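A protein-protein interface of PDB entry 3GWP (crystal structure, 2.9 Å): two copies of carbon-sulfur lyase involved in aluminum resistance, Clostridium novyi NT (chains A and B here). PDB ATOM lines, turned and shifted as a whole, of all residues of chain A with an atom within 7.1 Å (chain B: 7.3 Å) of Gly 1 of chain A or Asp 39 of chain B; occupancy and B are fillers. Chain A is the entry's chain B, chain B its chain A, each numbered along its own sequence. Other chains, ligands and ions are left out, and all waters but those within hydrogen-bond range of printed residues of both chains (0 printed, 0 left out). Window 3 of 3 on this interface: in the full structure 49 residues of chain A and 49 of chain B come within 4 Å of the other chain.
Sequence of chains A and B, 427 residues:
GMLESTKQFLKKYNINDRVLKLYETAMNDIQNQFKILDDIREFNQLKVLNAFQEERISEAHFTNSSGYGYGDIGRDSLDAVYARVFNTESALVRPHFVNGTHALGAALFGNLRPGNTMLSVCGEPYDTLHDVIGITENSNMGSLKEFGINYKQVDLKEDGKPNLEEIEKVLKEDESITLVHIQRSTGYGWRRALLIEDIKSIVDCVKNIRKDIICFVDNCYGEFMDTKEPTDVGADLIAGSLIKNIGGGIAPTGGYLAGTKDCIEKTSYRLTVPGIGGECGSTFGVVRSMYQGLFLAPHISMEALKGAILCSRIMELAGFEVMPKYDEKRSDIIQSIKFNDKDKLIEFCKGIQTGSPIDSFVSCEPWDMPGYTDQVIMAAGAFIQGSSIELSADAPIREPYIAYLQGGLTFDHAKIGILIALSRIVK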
ATOM      1  N   GLY A   1       4.960 -28.034 -17.250  1.00  0.00           N
ATOM      2  CA  GLY A   1       4.281 -29.248 -16.723  1.00  0.00           C
ATOM      3  C   GLY A   1       3.832 -29.063 -15.289  1.00  0.00           C
ATOM      4  O   GLY A   1       4.383 -28.240 -14.559  1.00  0.00           O
ATOM      5  N   MET A   2       2.839 -29.850 -14.882  1.00  0.00           N
ATOM      6  CA  MET A   2       2.278 -29.784 -13.525  1.00  0.00           C
ATOM      7  C   MET A   2       3.359 -30.037 -12.469  1.00  0.00           C
ATOM      8  O   MET A   2       4.197 -30.918 -12.642  1.00  0.00           O
ATOM      9  CB  MET A   2       1.140 -30.817 -13.387  1.00  0.00           C
ATOM     10  CG  MET A   2       0.402 -30.827 -12.041  1.00  0.00           C
ATOM     11  SD  MET A   2      -1.025 -32.175 -12.012  1.00  0.00           S
ATOM     12  CE  MET A   2      -2.160 -31.430 -13.425  1.00  0.00           C
ATOM     13  N   LEU A   3       3.347 -29.235 -11.400  1.00  0.00           N
ATOM     14  CA  LEU A   3       4.318 -29.373 -10.308  1.00  0.00           C
ATOM     15  C   LEU A   3       4.051 -30.635  -9.484  1.00  0.00           C
ATOM     16  O   LEU A   3       2.923 -31.126  -9.430  1.00  0.00           O
ATOM     17  CB  LEU A   3       4.278 -28.143  -9.382  1.00  0.00           C
ATOM     18  CG  LEU A   3       4.744 -26.795  -9.951  1.00  0.00           C
ATOM     19  CD1 LEU A   3       4.466 -25.667  -8.960  1.00  0.00           C
ATOM     20  CD2 LEU A   3       6.231 -26.834 -10.321  1.00  0.00           C
ATOM     21  N   GLU A   4       5.102 -31.151  -8.845  1.00  0.00           N
ATOM     22  CA  GLU A   4       4.985 -32.342  -7.998  1.00  0.00           C
ATOM     23  C   GLU A   4       4.082 -32.066  -6.788  1.00  0.00           C
ATOM     24  O   GLU A   4       3.339 -32.943  -6.364  1.00  0.00           O
ATOM     25  CB  GLU A   4       6.365 -32.817  -7.535  1.00  0.00           C
ATOM     26  N   SER A   5       4.139 -30.837  -6.259  1.00  0.00           N
ATOM     27  CA  SER A   5       3.297 -30.439  -5.111  1.00  0.00           C
ATOM     28  C   SER A   5       1.813 -30.270  -5.487  1.00  0.00           C
ATOM     29  O   SER A   5       0.947 -30.363  -4.620  1.00  0.00           O
ATOM     30  CB  SER A   5       3.818 -29.148  -4.472  1.00  0.00           C
ATOM     31  OG  SER A   5       3.822 -28.083  -5.396  1.00  0.00           O
ATOM     32  N   THR A   6       1.533 -30.001  -6.770  1.00  0.00           N
ATOM     33  CA  THR A   6       0.157 -29.839  -7.252  1.00  0.00           C
ATOM     34  C   THR A   6      -0.553 -31.178  -7.314  1.00  0.00           C
ATOM     35  O   THR A   6      -1.634 -31.333  -6.749  1.00  0.00           O
ATOM     36  CB  THR A   6       0.109 -29.209  -8.648  1.00  0.00           C
ATOM     37  OG1 THR A   6       0.701 -27.908  -8.609  1.00  0.00           O
ATOM     38  CG2 THR A   6      -1.339 -29.101  -9.137  1.00  0.00           C
ATOM     39  N   GLU A  24      -2.826 -35.554 -19.151  1.00  0.00           N
ATOM     40  CA  GLU A  24      -1.600 -35.104 -19.866  1.00  0.00           C
ATOM     41  C   GLU A  24      -1.637 -35.362 -21.379  1.00  0.00           C
ATOM     42  O   GLU A  24      -1.023 -34.619 -22.148  1.00  0.00           O
ATOM     43  CB  GLU A  24      -0.327 -35.735 -19.257  1.00  0.00           C
ATOM     44  CG  GLU A  24       0.109 -35.158 -17.869  1.00  0.00           C
ATOM     45  CD  GLU A  24       0.608 -33.682 -17.930  1.00  0.00           C
ATOM     46  OE1 GLU A  24       0.781 -33.137 -19.049  1.00  0.00           O
ATOM     47  OE2 GLU A  24       0.836 -33.080 -16.850  1.00  0.00           O
ATOM     48  N   ASP A 412      -7.988 -23.103 -15.018  1.00  0.00           N
ATOM     49  CA  ASP A 412      -7.513 -23.952 -13.923  1.00  0.00           C
ATOM     50  C   ASP A 412      -8.674 -24.486 -13.082  1.00  0.00           C
ATOM     51  O   ASP A 412      -8.685 -25.659 -12.725  1.00  0.00           O
ATOM     52  CB  ASP A 412      -6.515 -23.185 -13.031  1.00  0.00           C
ATOM     53  CG  ASP A 412      -5.167 -22.941 -13.719  1.00  0.00           C
ATOM     54  OD1 ASP A 412      -4.525 -23.924 -14.166  1.00  0.00           O
ATOM     55  OD2 ASP A 412      -4.723 -21.774 -13.751  1.00  0.00           O
ATOM     56  N   LYS A 415     -10.453 -27.078 -15.104  1.00  0.00           N
ATOM     57  CA  LYS A 415      -9.527 -28.223 -15.087  1.00  0.00           C
ATOM     58  C   LYS A 415      -9.607 -29.004 -13.764  1.00  0.00           C
ATOM     59  O   LYS A 415      -9.731 -30.233 -13.776  1.00  0.00           O
ATOM     60  CB  LYS A 415      -8.086 -27.733 -15.364  1.00  0.00           C
ATOM     61  CG  LYS A 415      -6.967 -28.724 -15.026  1.00  0.00           C
ATOM     62  CD  LYS A 415      -5.608 -28.301 -15.621  1.00  0.00           C
ATOM     63  CE  LYS A 415      -5.145 -26.915 -15.164  1.00  0.00           C
ATOM     64  NZ  LYS A 415      -3.793 -26.560 -15.698  1.00  0.00           N
ATOM     65  N   ASN B  32       8.630 -20.107 -22.862  1.00  0.00           N
ATOM     66  CA  ASN B  32       9.018 -21.016 -21.755  1.00  0.00           C
ATOM     67  C   ASN B  32       8.798 -20.412 -20.361  1.00  0.00           C
ATOM     68  O   ASN B  32       8.427 -21.121 -19.426  1.00  0.00           O
ATOM     69  CB  ASN B  32      10.483 -21.459 -21.910  1.00  0.00           C
ATOM     70  CG  ASN B  32      10.709 -22.340 -23.140  1.00  0.00           C
ATOM     71  OD1 ASN B  32       9.888 -23.197 -23.466  1.00  0.00           O
ATOM     72  ND2 ASN B  32      11.846 -22.153 -23.802  1.00  0.00           N
ATOM     73  N   PHE B  34       6.458 -18.220 -19.568  1.00  0.00           N
ATOM     74  CA  PHE B  34       4.987 -18.248 -19.362  1.00  0.00           C
ATOM     75  C   PHE B  34       4.507 -19.622 -18.880  1.00  0.00           C
ATOM     76  O   PHE B  34       3.563 -19.710 -18.092  1.00  0.00           O
ATOM     77  CB  PHE B  34       4.247 -17.861 -20.657  1.00  0.00           C
ATOM     78  CG  PHE B  34       4.122 -16.366 -20.882  1.00  0.00           C
ATOM     79  CD1 PHE B  34       5.185 -15.498 -20.632  1.00  0.00           C
ATOM     80  CD2 PHE B  34       2.978 -15.850 -21.478  1.00  0.00           C
ATOM     81  CE1 PHE B  34       5.060 -14.132 -20.877  1.00  0.00           C
ATOM     82  CE2 PHE B  34       2.858 -14.489 -21.740  1.00  0.00           C
ATOM     83  CZ  PHE B  34       3.900 -13.633 -21.443  1.00  0.00           C
ATOM     84  N   LYS B  35       5.145 -20.689 -19.380  1.00  0.00           N
ATOM     85  CA  LYS B  35       4.819 -22.056 -18.959  1.00  0.00           C
ATOM     86  C   LYS B  35       5.190 -22.282 -17.474  1.00  0.00           C
ATOM     87  O   LYS B  35       4.506 -23.036 -16.764  1.00  0.00           O
ATOM     88  CB  LYS B  35       5.507 -23.093 -19.864  1.00  0.00           C
ATOM     89  CG  LYS B  35       5.005 -23.082 -21.312  1.00  0.00           C
ATOM     90  CD  LYS B  35       5.691 -24.144 -22.158  1.00  0.00           C
ATOM     91  N   ILE B  36       6.269 -21.633 -17.019  1.00  0.00           N
ATOM     92  CA  ILE B  36       6.686 -21.714 -15.616  1.00  0.00           C
ATOM     93  C   ILE B  36       5.657 -21.004 -14.711  1.00  0.00           C
ATOM     94  O   ILE B  36       5.453 -21.409 -13.569  1.00  0.00           O
ATOM     95  CB  ILE B  36       8.084 -21.094 -15.395  1.00  0.00           C
ATOM     96  N   LEU B  37       5.036 -19.935 -15.227  1.00  0.00           N
ATOM     97  CA  LEU B  37       3.981 -19.198 -14.489  1.00  0.00           C
ATOM     98  C   LEU B  37       2.666 -19.985 -14.437  1.00  0.00           C
ATOM     99  O   LEU B  37       1.956 -19.937 -13.430  1.00  0.00           O
ATOM    100  CB  LEU B  37       3.717 -17.815 -15.117  1.00  0.00           C
ATOM    101  CG  LEU B  37       4.671 -16.647 -14.815  1.00  0.00           C
ATOM    102  CD1 LEU B  37       6.134 -16.996 -15.017  1.00  0.00           C
ATOM    103  CD2 LEU B  37       4.277 -15.442 -15.663  1.00  0.00           C
ATOM    104  N   ASP B  38       2.334 -20.677 -15.537  1.00  0.00           N
ATOM    105  CA  ASP B  38       1.087 -21.472 -15.630  1.00  0.00           C
ATOM    106  C   ASP B  38       1.022 -22.634 -14.636  1.00  0.00           C
ATOM    107  O   ASP B  38      -0.054 -22.936 -14.116  1.00  0.00           O
ATOM    108  CB  ASP B  38       0.879 -22.016 -17.060  1.00  0.00           C
ATOM    109  CG  ASP B  38       0.563 -20.920 -18.076  1.00  0.00           C
ATOM    110  OD1 ASP B  38       0.181 -19.801 -17.673  1.00  0.00           O
ATOM    111  OD2 ASP B  38       0.664 -21.199 -19.285  1.00  0.00           O
ATOM    112  N   ASP B  39       2.151 -23.302 -14.390  1.00  0.00           N
ATOM    113  CA  ASP B  39       2.160 -24.423 -13.423  1.00  0.00           C
ATOM    114  C   ASP B  39       2.271 -23.952 -11.950  1.00  0.00           C
ATOM    115  O   ASP B  39       2.050 -24.743 -11.032  1.00  0.00           O
ATOM    116  CB  ASP B  39       3.177 -25.546 -13.807  1.00  0.00           C
ATOM    117  CG  ASP B  39       4.588 -25.037 -14.037  1.00  0.00           C
ATOM    118  OD1 ASP B  39       5.129 -24.325 -13.166  1.00  0.00           O
ATOM    119  OD2 ASP B  39       5.188 -25.430 -15.062  1.00  0.00           O
ATOM    120  N   ILE B  40       2.591 -22.664 -11.739  1.00  0.00           N
ATOM    121  CA  ILE B  40       2.590 -22.058 -10.382  1.00  0.00           C
ATOM    122  C   ILE B  40       1.163 -21.572 -10.072  1.00  0.00           C
ATOM    123  O   ILE B  40       0.674 -21.709  -8.944  1.00  0.00           O
ATOM    124  CB  ILE B  40       3.571 -20.872 -10.261  1.00  0.00           C
ATOM    125  CG1 ILE B  40       5.013 -21.368 -10.270  1.00  0.00           C
ATOM    126  CG2 ILE B  40       3.337 -20.116  -8.965  1.00  0.00           C
ATOM    127  CD1 ILE B  40       6.052 -20.245 -10.222  1.00  0.00           C
ATOM    128  N   ARG B  41       0.527 -20.963 -11.081  1.00  0.00           N
ATOM    129  CA  ARG B  41      -0.860 -20.481 -10.996  1.00  0.00           C
ATOM    130  C   ARG B  41      -1.839 -21.629 -10.673  1.00  0.00           C
ATOM    131  O   ARG B  41      -2.793 -21.455  -9.893  1.00  0.00           O
ATOM    132  CB  ARG B  41      -1.244 -19.843 -12.334  1.00  0.00           C
ATOM    133  CG  ARG B  41      -2.709 -19.397 -12.455  1.00  0.00           C
ATOM    134  CD  ARG B  41      -2.995 -18.787 -13.816  1.00  0.00           C
ATOM    135  NE  ARG B  41      -2.820 -19.732 -14.922  1.00  0.00           N
ATOM    136  CZ  ARG B  41      -2.939 -19.416 -16.216  1.00  0.00           C
ATOM    137  NH1 ARG B  41      -3.220 -18.157 -16.598  1.00  0.00           N
ATOM    138  NH2 ARG B  41      -2.756 -20.356 -17.144  1.00  0.00           N
ATOM    139  N   GLU B  42      -1.607 -22.776 -11.327  1.00  0.00           N
ATOM    140  CA  GLU B  42      -2.408 -23.993 -11.161  1.00  0.00           C
ATOM    141  C   GLU B  42      -2.503 -24.375  -9.697  1.00  0.00           C
ATOM    142  O   GLU B  42      -3.601 -24.601  -9.180  1.00  0.00           O
ATOM    143  CB  GLU B  42      -1.765 -25.137 -11.958  1.00  0.00           C
ATOM    144  CG  GLU B  42      -2.567 -26.425 -12.029  1.00  0.00           C
ATOM    145  CD  GLU B  42      -1.903 -27.460 -12.915  1.00  0.00           C
ATOM    146  OE1 GLU B  42      -0.652 -27.505 -12.953  1.00  0.00           O
ATOM    147  OE2 GLU B  42      -2.626 -28.247 -13.561  1.00  0.00           O
ATOM    148  N   PHE B  43      -1.342 -24.435  -9.035  1.00  0.00           N
ATOM    149  CA  PHE B  43      -1.265 -24.757  -7.606  1.00  0.00           C
ATOM    150  C   PHE B  43      -2.000 -23.724  -6.762  1.00  0.00           C
ATOM    151  O   PHE B  43      -2.685 -24.081  -5.811  1.00  0.00           O
ATOM    152  CB  PHE B  43       0.192 -24.818  -7.154  1.00  0.00           C
ATOM    153  CG  PHE B  43       0.365 -25.170  -5.701  1.00  0.00           C
ATOM    154  CD1 PHE B  43       0.511 -26.493  -5.308  1.00  0.00           C
ATOM    155  CD2 PHE B  43       0.401 -24.175  -4.725  1.00  0.00           C
ATOM    156  CE1 PHE B  43       0.680 -26.822  -3.966  1.00  0.00           C
ATOM    157  CE2 PHE B  43       0.559 -24.499  -3.385  1.00  0.00           C
ATOM    158  CZ  PHE B  43       0.703 -25.825  -3.006  1.00  0.00           C
ATOM    159  N   ASN B  44      -1.818 -22.441  -7.091  1.00  0.00           N
ATOM    160  CA  ASN B  44      -2.466 -21.351  -6.347  1.00  0.00           C
ATOM    161  C   ASN B  44      -3.988 -21.359  -6.471  1.00  0.00           C
ATOM    162  O   ASN B  44      -4.685 -21.027  -5.511  1.00  0.00           O
ATOM    163  CB  ASN B  44      -1.903 -19.980  -6.766  1.00  0.00           C
ATOM    164  CG  ASN B  44      -0.455 -19.765  -6.311  1.00  0.00           C
ATOM    165  OD1 ASN B  44       0.017 -20.391  -5.359  1.00  0.00           O
ATOM    166  ND2 ASN B  44       0.232 -18.834  -6.963  1.00  0.00           N
ATOM    167  N   THR B 227       4.450 -20.382  -5.417  1.00  0.00           N
ATOM    168  CA  THR B 227       3.587 -21.393  -4.781  1.00  0.00           C
ATOM    169  C   THR B 227       3.526 -21.196  -3.260  1.00  0.00           C
ATOM    170  O   THR B 227       2.468 -21.349  -2.656  1.00  0.00           O
ATOM    171  CB  THR B 227       4.059 -22.826  -5.088  1.00  0.00           C
ATOM    172  OG1 THR B 227       5.426 -22.985  -4.679  1.00  0.00           O
ATOM    173  CG2 THR B 227       3.931 -23.121  -6.579  1.00  0.00           C
ATOM    174  N   MET B 302      -1.087 -13.428 -12.530  1.00  0.00           N
ATOM    175  CA  MET B 302      -0.210 -13.859 -13.623  1.00  0.00           C
ATOM    176  C   MET B 302      -0.509 -13.177 -14.959  1.00  0.00           C
ATOM    177  O   MET B 302       0.338 -13.185 -15.840  1.00  0.00           O
ATOM    178  CB  MET B 302      -0.242 -15.379 -13.787  1.00  0.00           C
ATOM    179  CG  MET B 302       0.294 -16.148 -12.580  1.00  0.00           C
ATOM    180  SD  MET B 302       2.047 -15.538 -11.992  1.00  0.00           S
ATOM    181  CE  MET B 302       2.463 -16.966 -10.717  1.00  0.00           C
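Among the printed residues, pairs that only touch across the chains: Met 2 of chain A with Glu 42 of chain B (3.2 Å), Leu 3 of chain A with Asp 39 of chain B (3.3 Å), Leu 3 of chain A with Thr 227 of chain B (3.5 Å), Ser 5 of chain A with Phe 43 of chain B (3.6 Å), Thr 6 of chain A with Phe 43 of chain B (3.5 Å) and Asp 412 of chain A with Glu 42 of chain B (3.7 Å).
Of the 14 printed residues of chain B, 5 touch a printed residue of chain A.
Among the printed residues, Asp or Glu carboxylates within 4 Å of a Lys or Arg side-chain nitrogen of the other chain: Asp 412 of chain A with Arg 41 of chain B (3.0 Å) and Lys 415 of chain A with Glu 42 of chain B (3.0 Å).
No position is printed for both chains.
The side-chain carboxylate (OD2) of Asp 39 of chain B is in hydrogen-bond range of the backbone NH (N) of Gly 1 of chain A, at 3.4 Å.
The side-chain carboxylate (OD2) of Asp 412 of chain A is in salt-bridge range of the guanidinium group (NE) of Arg 41 of chain B (3.0 Å).
NZ of Lys 415 of chain A is in salt-bridge range of OE2 of Glu 42 of chain B.
Gly 1 of chain A touches just one residue of chain B: Asp 39 (3.0 Å).
Asp 39 of chain B touches just these residues of chain A: Gly 1 and Leu 3.
Of the printed residues of chain B, Ser 5 of chain A touches Phe 43.
Of the printed residues of chain B, Asp 412 of chain A touches Arg 41 and Glu 42.
Of the printed residues of chain A, Arg 41 of chain B touches Asp 412 (3.0 Å).
The nearest residue of chain B that does not touch Gly 1 of chain A is Lys 35 of chain B (5.0 Å).
OD1 of Asp 412 of chain A lies within salt-bridge range of NZ of Lys 415 of chain A (3.1 Å).
OD1 of Asp 38 of chain B lies within salt-bridge range of NH2 of Arg 41 of chain B (3.0 Å).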
